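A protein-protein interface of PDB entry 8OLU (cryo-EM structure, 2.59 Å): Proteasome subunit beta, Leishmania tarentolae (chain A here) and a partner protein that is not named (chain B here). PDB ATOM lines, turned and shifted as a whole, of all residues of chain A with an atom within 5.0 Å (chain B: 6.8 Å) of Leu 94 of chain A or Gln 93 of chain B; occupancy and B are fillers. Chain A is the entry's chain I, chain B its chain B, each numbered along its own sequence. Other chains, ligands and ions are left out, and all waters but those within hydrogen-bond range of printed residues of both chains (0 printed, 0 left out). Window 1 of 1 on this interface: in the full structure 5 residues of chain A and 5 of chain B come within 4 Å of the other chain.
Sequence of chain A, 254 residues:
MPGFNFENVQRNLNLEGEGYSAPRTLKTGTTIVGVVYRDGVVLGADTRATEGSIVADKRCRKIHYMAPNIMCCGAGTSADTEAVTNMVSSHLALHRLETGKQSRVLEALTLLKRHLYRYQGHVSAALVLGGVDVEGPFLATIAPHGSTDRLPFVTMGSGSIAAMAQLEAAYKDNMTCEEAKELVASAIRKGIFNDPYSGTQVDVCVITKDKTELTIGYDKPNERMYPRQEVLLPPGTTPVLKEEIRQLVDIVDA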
ATOM      1  N   SER A  90      25.246  17.735 -21.588  1.00  0.00           N
ATOM      2  CA  SER A  90      25.106  19.166 -21.707  1.00  0.00           C
ATOM      3  C   SER A  90      25.642  19.849 -20.486  1.00  0.00           C
ATOM      4  O   SER A  90      26.375  20.782 -20.602  1.00  0.00           O
ATOM      5  CB  SER A  90      23.687  19.551 -21.862  1.00  0.00           C
ATOM      6  OG  SER A  90      23.562  20.984 -21.845  1.00  0.00           O
ATOM      7  N   HIS A  91      25.260  19.399 -19.312  1.00  0.00           N
ATOM      8  CA  HIS A  91      25.798  19.940 -18.090  1.00  0.00           C
ATOM      9  C   HIS A  91      27.329  19.885 -18.067  1.00  0.00           C
ATOM     10  O   HIS A  91      28.008  20.861 -17.844  1.00  0.00           O
ATOM     11  CB  HIS A  91      25.193  19.190 -16.941  1.00  0.00           C
ATOM     12  CG  HIS A  91      25.332  19.886 -15.629  1.00  0.00           C
ATOM     13  ND1 HIS A  91      24.585  19.536 -14.519  1.00  0.00           N
ATOM     14  CD2 HIS A  91      26.172  20.903 -15.253  1.00  0.00           C
ATOM     15  CE1 HIS A  91      24.919  20.339 -13.500  1.00  0.00           C
ATOM     16  NE2 HIS A  91      25.928  21.186 -13.940  1.00  0.00           N
ATOM     17  N   LEU A  92      27.915  18.765 -18.377  1.00  0.00           N
ATOM     18  CA  LEU A  92      29.334  18.737 -18.398  1.00  0.00           C
ATOM     19  C   LEU A  92      29.943  19.637 -19.439  1.00  0.00           C
ATOM     20  O   LEU A  92      31.074  20.079 -19.253  1.00  0.00           O
ATOM     21  CB  LEU A  92      29.794  17.350 -18.747  1.00  0.00           C
ATOM     22  CG  LEU A  92      29.444  16.249 -17.789  1.00  0.00           C
ATOM     23  CD1 LEU A  92      29.874  14.922 -18.416  1.00  0.00           C
ATOM     24  CD2 LEU A  92      30.093  16.429 -16.462  1.00  0.00           C
ATOM     25  N   ALA A  93      29.293  19.840 -20.568  1.00  0.00           N
ATOM     26  CA  ALA A  93      29.818  20.763 -21.578  1.00  0.00           C
ATOM     27  C   ALA A  93      29.943  22.159 -20.996  1.00  0.00           C
ATOM     28  O   ALA A  93      30.912  22.853 -21.195  1.00  0.00           O
ATOM     29  CB  ALA A  93      28.913  20.812 -22.750  1.00  0.00           C
ATOM     30  N   LEU A  94      28.940  22.501 -20.243  1.00  0.00           N
ATOM     31  CA  LEU A  94      28.801  23.778 -19.609  1.00  0.00           C
ATOM     32  C   LEU A  94      29.791  23.937 -18.484  1.00  0.00           C
ATOM     33  O   LEU A  94      30.315  24.996 -18.228  1.00  0.00           O
ATOM     34  CB  LEU A  94      27.396  23.739 -19.041  1.00  0.00           C
ATOM     35  CG  LEU A  94      26.684  25.061 -18.921  1.00  0.00           C
ATOM     36  CD1 LEU A  94      26.698  25.763 -20.263  1.00  0.00           C
ATOM     37  CD2 LEU A  94      25.243  24.805 -18.502  1.00  0.00           C
ATOM     38  N   HIS A  95      29.975  22.858 -17.759  1.00  0.00           N
ATOM     39  CA  HIS A  95      30.824  22.856 -16.600  1.00  0.00           C
ATOM     40  C   HIS A  95      32.246  22.996 -17.070  1.00  0.00           C
ATOM     41  O   HIS A  95      33.068  23.497 -16.359  1.00  0.00           O
ATOM     42  CB  HIS A  95      30.613  21.563 -15.837  1.00  0.00           C
ATOM     43  CG  HIS A  95      31.314  21.576 -14.531  1.00  0.00           C
ATOM     44  ND1 HIS A  95      31.043  22.514 -13.582  1.00  0.00           N
ATOM     45  CD2 HIS A  95      32.372  20.813 -14.113  1.00  0.00           C
ATOM     46  CE1 HIS A  95      31.959  22.371 -12.626  1.00  0.00           C
ATOM     47  NE2 HIS A  95      32.792  21.311 -12.920  1.00  0.00           N
ATOM     48  N   ARG A  96      32.521  22.452 -18.248  1.00  0.00           N
ATOM     49  CA  ARG A  96      33.830  22.534 -18.851  1.00  0.00           C
ATOM     50  C   ARG A  96      34.165  23.930 -19.270  1.00  0.00           C
ATOM     51  O   ARG A  96      35.342  24.200 -19.416  1.00  0.00           O
ATOM     52  CB  ARG A  96      33.948  21.817 -20.192  1.00  0.00           C
ATOM     53  CG  ARG A  96      34.460  20.405 -20.049  1.00  0.00           C
ATOM     54  CD  ARG A  96      35.012  19.797 -21.272  1.00  0.00           C
ATOM     55  NE  ARG A  96      34.003  19.669 -22.292  1.00  0.00           N
ATOM     56  CZ  ARG A  96      32.939  18.869 -22.264  1.00  0.00           C
ATOM     57  NH1 ARG A  96      32.632  18.075 -21.251  1.00  0.00           N
ATOM     58  NH2 ARG A  96      32.147  18.931 -23.303  1.00  0.00           N
ATOM     59  N   LEU A  97      33.175  24.744 -19.633  1.00  0.00           N
ATOM     60  CA  LEU A  97      33.472  26.133 -19.960  1.00  0.00           C
ATOM     61  C   LEU A  97      33.696  26.907 -18.675  1.00  0.00           C
ATOM     62  O   LEU A  97      34.647  27.631 -18.612  1.00  0.00           O
ATOM     63  CB  LEU A  97      32.322  26.720 -20.728  1.00  0.00           C
ATOM     64  CG  LEU A  97      32.097  26.052 -22.063  1.00  0.00           C
ATOM     65  CD1 LEU A  97      30.813  26.509 -22.679  1.00  0.00           C
ATOM     66  CD2 LEU A  97      33.248  26.354 -22.986  1.00  0.00           C
ATOM     67  N   GLU A  98      32.927  26.647 -17.631  1.00  0.00           N
ATOM     68  CA  GLU A  98      33.142  27.276 -16.338  1.00  0.00           C
ATOM     69  C   GLU A  98      34.572  27.009 -15.864  1.00  0.00           C
ATOM     70  O   GLU A  98      35.304  27.973 -15.699  1.00  0.00           O
ATOM     71  CB  GLU A  98      32.026  26.858 -15.360  1.00  0.00           C
ATOM     72  CG  GLU A  98      32.155  27.387 -13.926  1.00  0.00           C
ATOM     73  CD  GLU A  98      31.045  26.957 -12.945  1.00  0.00           C
ATOM     74  OE1 GLU A  98      30.781  25.704 -12.856  1.00  0.00           O
ATOM     75  OE2 GLU A  98      30.458  27.848 -12.222  1.00  0.00           O
ATOM     76  N   LEU B  66      31.158  30.342 -25.928  1.00  0.00           N
ATOM     77  CA  LEU B  66      29.803  30.138 -25.456  1.00  0.00           C
ATOM     78  C   LEU B  66      29.292  28.756 -25.874  1.00  0.00           C
ATOM     79  O   LEU B  66      28.529  28.094 -25.182  1.00  0.00           O
ATOM     80  CB  LEU B  66      28.951  31.209 -26.105  1.00  0.00           C
ATOM     81  CG  LEU B  66      29.442  32.623 -25.932  1.00  0.00           C
ATOM     82  CD1 LEU B  66      28.463  33.584 -26.525  1.00  0.00           C
ATOM     83  CD2 LEU B  66      29.507  32.975 -24.488  1.00  0.00           C
ATOM     84  N   ASP B  67      29.705  28.324 -27.042  1.00  0.00           N
ATOM     85  CA  ASP B  67      29.493  26.959 -27.419  1.00  0.00           C
ATOM     86  C   ASP B  67      30.500  26.643 -28.497  1.00  0.00           C
ATOM     87  O   ASP B  67      31.308  27.472 -28.809  1.00  0.00           O
ATOM     88  CB  ASP B  67      28.062  26.744 -27.889  1.00  0.00           C
ATOM     89  CG  ASP B  67      27.610  25.271 -27.846  1.00  0.00           C
ATOM     90  OD1 ASP B  67      28.410  24.376 -27.362  1.00  0.00           O
ATOM     91  OD2 ASP B  67      26.456  24.998 -28.278  1.00  0.00           O
ATOM     92  N   GLU B  68      30.490  25.448 -29.025  1.00  0.00           N
ATOM     93  CA  GLU B  68      31.475  25.038 -29.994  1.00  0.00           C
ATOM     94  C   GLU B  68      31.539  26.057 -31.105  1.00  0.00           C
ATOM     95  O   GLU B  68      32.611  26.417 -31.551  1.00  0.00           O
ATOM     96  CB  GLU B  68      31.153  23.634 -30.515  1.00  0.00           C
ATOM     97  CG  GLU B  68      31.390  22.506 -29.477  1.00  0.00           C
ATOM     98  CD  GLU B  68      30.912  21.073 -29.799  1.00  0.00           C
ATOM     99  OE1 GLU B  68      29.666  20.805 -29.791  1.00  0.00           O
ATOM    100  OE2 GLU B  68      31.783  20.206 -30.070  1.00  0.00           O
ATOM    101  N   ASP B  86      27.446  33.587 -18.725  1.00  0.00           N
ATOM    102  CA  ASP B  86      26.931  32.388 -18.106  1.00  0.00           C
ATOM    103  C   ASP B  86      25.569  32.095 -18.673  1.00  0.00           C
ATOM    104  O   ASP B  86      25.292  30.951 -19.040  1.00  0.00           O
ATOM    105  CB  ASP B  86      26.955  32.483 -16.595  1.00  0.00           C
ATOM    106  CG  ASP B  86      28.353  32.247 -15.995  1.00  0.00           C
ATOM    107  OD1 ASP B  86      29.279  31.651 -16.732  1.00  0.00           O
ATOM    108  OD2 ASP B  86      28.555  32.703 -14.791  1.00  0.00           O
ATOM    109  N   ALA B  88      24.291  32.982 -21.568  1.00  0.00           N
ATOM    110  CA  ALA B  88      24.367  32.673 -22.961  1.00  0.00           C
ATOM    111  C   ALA B  88      24.864  31.257 -23.165  1.00  0.00           C
ATOM    112  O   ALA B  88      24.502  30.570 -24.117  1.00  0.00           O
ATOM    113  CB  ALA B  88      25.313  33.604 -23.619  1.00  0.00           C
ATOM    114  N   ARG B  89      25.738  30.810 -22.279  1.00  0.00           N
ATOM    115  CA  ARG B  89      26.193  29.450 -22.348  1.00  0.00           C
ATOM    116  C   ARG B  89      25.039  28.543 -22.051  1.00  0.00           C
ATOM    117  O   ARG B  89      24.885  27.551 -22.690  1.00  0.00           O
ATOM    118  CB  ARG B  89      27.323  29.307 -21.365  1.00  0.00           C
ATOM    119  CG  ARG B  89      28.664  29.685 -21.942  1.00  0.00           C
ATOM    120  CD  ARG B  89      29.575  29.977 -20.810  1.00  0.00           C
ATOM    121  NE  ARG B  89      30.925  30.041 -21.282  1.00  0.00           N
ATOM    122  CZ  ARG B  89      31.897  30.335 -20.463  1.00  0.00           C
ATOM    123  NH1 ARG B  89      31.633  30.280 -19.160  1.00  0.00           N
ATOM    124  NH2 ARG B  89      33.057  30.711 -20.965  1.00  0.00           N
ATOM    125  N   LYS B  90      24.268  28.867 -21.027  1.00  0.00           N
ATOM    126  CA  LYS B  90      23.120  28.039 -20.718  1.00  0.00           C
ATOM    127  C   LYS B  90      22.184  27.966 -21.900  1.00  0.00           C
ATOM    128  O   LYS B  90      21.702  26.893 -22.191  1.00  0.00           O
ATOM    129  CB  LYS B  90      22.324  28.563 -19.550  1.00  0.00           C
ATOM    130  CG  LYS B  90      22.793  28.061 -18.203  1.00  0.00           C
ATOM    131  CD  LYS B  90      21.701  28.273 -17.169  1.00  0.00           C
ATOM    132  CE  LYS B  90      20.323  27.879 -17.696  1.00  0.00           C
ATOM    133  NZ  LYS B  90      19.346  27.642 -16.603  1.00  0.00           N
ATOM    134  N   ASN B  91      21.961  29.073 -22.574  1.00  0.00           N
ATOM    135  CA  ASN B  91      20.991  29.131 -23.625  1.00  0.00           C
ATOM    136  C   ASN B  91      21.475  28.311 -24.791  1.00  0.00           C
ATOM    137  O   ASN B  91      20.698  27.613 -25.415  1.00  0.00           O
ATOM    138  CB  ASN B  91      20.778  30.539 -24.161  1.00  0.00           C
ATOM    139  CG  ASN B  91      20.062  31.450 -23.190  1.00  0.00           C
ATOM    140  OD1 ASN B  91      19.109  31.031 -22.550  1.00  0.00           O
ATOM    141  ND2 ASN B  91      20.473  32.707 -23.109  1.00  0.00           N
ATOM    142  N   CYS B  92      22.734  28.452 -25.145  1.00  0.00           N
ATOM    143  CA  CYS B  92      23.259  27.571 -26.157  1.00  0.00           C
ATOM    144  C   CYS B  92      22.972  26.113 -25.854  1.00  0.00           C
ATOM    145  O   CYS B  92      22.804  25.341 -26.771  1.00  0.00           O
ATOM    146  CB  CYS B  92      24.765  27.656 -26.238  1.00  0.00           C
ATOM    147  SG  CYS B  92      25.330  29.248 -26.853  1.00  0.00           S
ATOM    148  N   GLN B  93      23.116  25.708 -24.600  1.00  0.00           N
ATOM    149  CA  GLN B  93      22.977  24.324 -24.260  1.00  0.00           C
ATOM    150  C   GLN B  93      21.492  23.987 -24.213  1.00  0.00           C
ATOM    151  O   GLN B  93      21.130  22.896 -24.605  1.00  0.00           O
ATOM    152  CB  GLN B  93      23.652  23.964 -22.942  1.00  0.00           C
ATOM    153  CG  GLN B  93      25.165  23.790 -22.986  1.00  0.00           C
ATOM    154  CD  GLN B  93      25.647  22.741 -23.945  1.00  0.00           C
ATOM    155  OE1 GLN B  93      25.120  21.624 -24.027  1.00  0.00           O
ATOM    156  NE2 GLN B  93      26.618  23.123 -24.760  1.00  0.00           N
ATOM    157  N   GLN B  94      20.640  24.861 -23.693  1.00  0.00           N
ATOM    158  CA  GLN B  94      19.231  24.550 -23.679  1.00  0.00           C
ATOM    159  C   GLN B  94      18.738  24.314 -25.076  1.00  0.00           C
ATOM    160  O   GLN B  94      17.986  23.397 -25.310  1.00  0.00           O
ATOM    161  CB  GLN B  94      18.375  25.637 -23.074  1.00  0.00           C
ATOM    162  CG  GLN B  94      18.553  25.669 -21.566  1.00  0.00           C
ATOM    163  CD  GLN B  94      17.667  26.756 -21.005  1.00  0.00           C
ATOM    164  OE1 GLN B  94      16.454  26.554 -20.867  1.00  0.00           O
ATOM    165  NE2 GLN B  94      18.249  27.938 -20.768  1.00  0.00           N
ATOM    166  N   TYR B  95      19.219  25.095 -26.000  1.00  0.00           N
ATOM    167  CA  TYR B  95      18.800  24.977 -27.362  1.00  0.00           C
ATOM    168  C   TYR B  95      19.256  23.664 -27.930  1.00  0.00           C
ATOM    169  O   TYR B  95      18.580  23.092 -28.722  1.00  0.00           O
ATOM    170  CB  TYR B  95      19.427  26.114 -28.148  1.00  0.00           C
ATOM    171  CG  TYR B  95      18.862  26.279 -29.511  1.00  0.00           C
ATOM    172  CD1 TYR B  95      17.875  27.190 -29.822  1.00  0.00           C
ATOM    173  CD2 TYR B  95      19.324  25.472 -30.528  1.00  0.00           C
ATOM    174  CE1 TYR B  95      17.391  27.294 -31.114  1.00  0.00           C
ATOM    175  CE2 TYR B  95      18.904  25.633 -31.840  1.00  0.00           C
ATOM    176  CZ  TYR B  95      17.936  26.559 -32.139  1.00  0.00           C
ATOM    177  OH  TYR B  95      17.582  26.520 -33.479  1.00  0.00           O
ATOM    178  N   LYS B  96      20.476  23.239 -27.686  1.00  0.00           N
ATOM    179  CA  LYS B  96      20.884  21.951 -28.180  1.00  0.00           C
ATOM    180  C   LYS B  96      20.040  20.861 -27.567  1.00  0.00           C
ATOM    181  O   LYS B  96      19.710  19.887 -28.197  1.00  0.00           O
ATOM    182  CB  LYS B  96      22.311  21.669 -27.777  1.00  0.00           C
ATOM    183  CG  LYS B  96      23.245  21.525 -28.936  1.00  0.00           C
ATOM    184  CD  LYS B  96      24.658  21.912 -28.575  1.00  0.00           C
ATOM    185  CE  LYS B  96      25.577  21.845 -29.778  1.00  0.00           C
ATOM    186  NZ  LYS B  96      26.731  22.763 -29.600  1.00  0.00           N
ATOM    187  N   LEU B  97      19.787  20.951 -26.291  1.00  0.00           N
ATOM    188  CA  LEU B  97      18.979  19.942 -25.693  1.00  0.00           C
ATOM    189  C   LEU B  97      17.644  19.885 -26.383  1.00  0.00           C
ATOM    190  O   LEU B  97      17.066  18.820 -26.458  1.00  0.00           O
ATOM    191  CB  LEU B  97      18.715  20.243 -24.235  1.00  0.00           C
ATOM    192  CG  LEU B  97      19.823  19.818 -23.291  1.00  0.00           C
ATOM    193  CD1 LEU B  97      19.433  20.250 -21.898  1.00  0.00           C
ATOM    194  CD2 LEU B  97      20.066  18.328 -23.312  1.00  0.00           C
ATOM    195  N   MET B  98      17.104  21.018 -26.792  1.00  0.00           N
ATOM    196  CA  MET B  98      15.823  20.946 -27.436  1.00  0.00           C
ATOM    197  C   MET B  98      15.941  20.532 -28.894  1.00  0.00           C
ATOM    198  O   MET B  98      15.275  19.641 -29.316  1.00  0.00           O
ATOM    199  CB  MET B  98      15.053  22.237 -27.364  1.00  0.00           C
ATOM    200  CG  MET B  98      13.589  22.011 -27.718  1.00  0.00           C
ATOM    201  SD  MET B  98      12.777  23.499 -27.196  1.00  0.00           S
ATOM    202  CE  MET B  98      12.757  23.267 -25.417  1.00  0.00           C
ATOM    203  N   ILE B 103      22.565  26.480 -31.475  1.00  0.00           N
ATOM    204  CA  ILE B 103      21.812  27.713 -31.533  1.00  0.00           C
ATOM    205  C   ILE B 103      22.394  28.644 -32.572  1.00  0.00           C
ATOM    206  O   ILE B 103      23.582  28.848 -32.616  1.00  0.00           O
ATOM    207  CB  ILE B 103      21.769  28.381 -30.170  1.00  0.00           C
ATOM    208  CG1 ILE B 103      20.563  29.279 -30.115  1.00  0.00           C
ATOM    209  CG2 ILE B 103      23.063  29.116 -29.875  1.00  0.00           C
ATOM    210  CD1 ILE B 103      20.455  30.055 -28.799  1.00  0.00           C
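The side-chain amide oxygen (OE1) of Gln 93 of chain B is in hydrogen-bond range of the side-chain hydroxyl (OG) of Ser 90 of chain A.
The side-chain sulfur (SG) of Cys 92 of chain B is in hydrogen-bond range of the backbone carbonyl oxygen (O) of Leu 66 of chain B (3.8 Å).
The side-chain amide nitrogen (NE2) of Gln 93 of chain B sits at hydrogen-bond distance from the side-chain carboxylate (OD1) of Asp 67 of chain B (3.4 Å).
The side-chain carboxylate (OD1) of Asp 86 of chain B lies within salt-bridge range of the guanidinium group (NH1) of Arg 89 of chain B, 3.6 Å away.
Ala 93 of chain A touches Gln 93 of chain B.
CD1 of Leu 94 of chain A touches O of Arg 89 of chain B, at 3.5 Å.
CG of Gln 93 of chain B touches CD1 of Leu 94 of chain A, 3.7 Å away.
O of Leu 66 of chain B touches CD1 of Leu 97 of chain A, at 3.7 Å.
Arg 89 of chain B touches Leu 97 of chain A.
Printed residues of chain B within 4 Å of Ser 90 of chain A: Gln 93 (2.8 Å).
Of the printed residues of chain B, Leu 94 of chain A touches Arg 89 (3.5 Å) and Gln 93 (3.7 Å).
Of the printed residues of chain B, Leu 97 of chain A touches Leu 66 (3.7 Å) and Arg 89 (3.6 Å).
Of the printed residues of chain A, Gln 93 of chain B touches Ser 90 (2.8 Å), Ala 93 (3.8 Å) and Leu 94 (3.7 Å).
The nearest printed residue of chain A that does not touch Gln 93 of chain B is His 91 of chain A (5.2 Å).
The nearest printed residue of chain B that does not touch Ser 90 of chain A is Leu 97 of chain B (4.1 Å).
Of the 9 printed residues of chain A, 4 touch a printed residue of chain B.
Hydrophobic or aromatic side chains of chain A that line the printed part of chain B: Ala 93, Leu 94 and Leu 97.
Of the 16 printed residues of chain B, 3 touch a printed residue of chain A.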
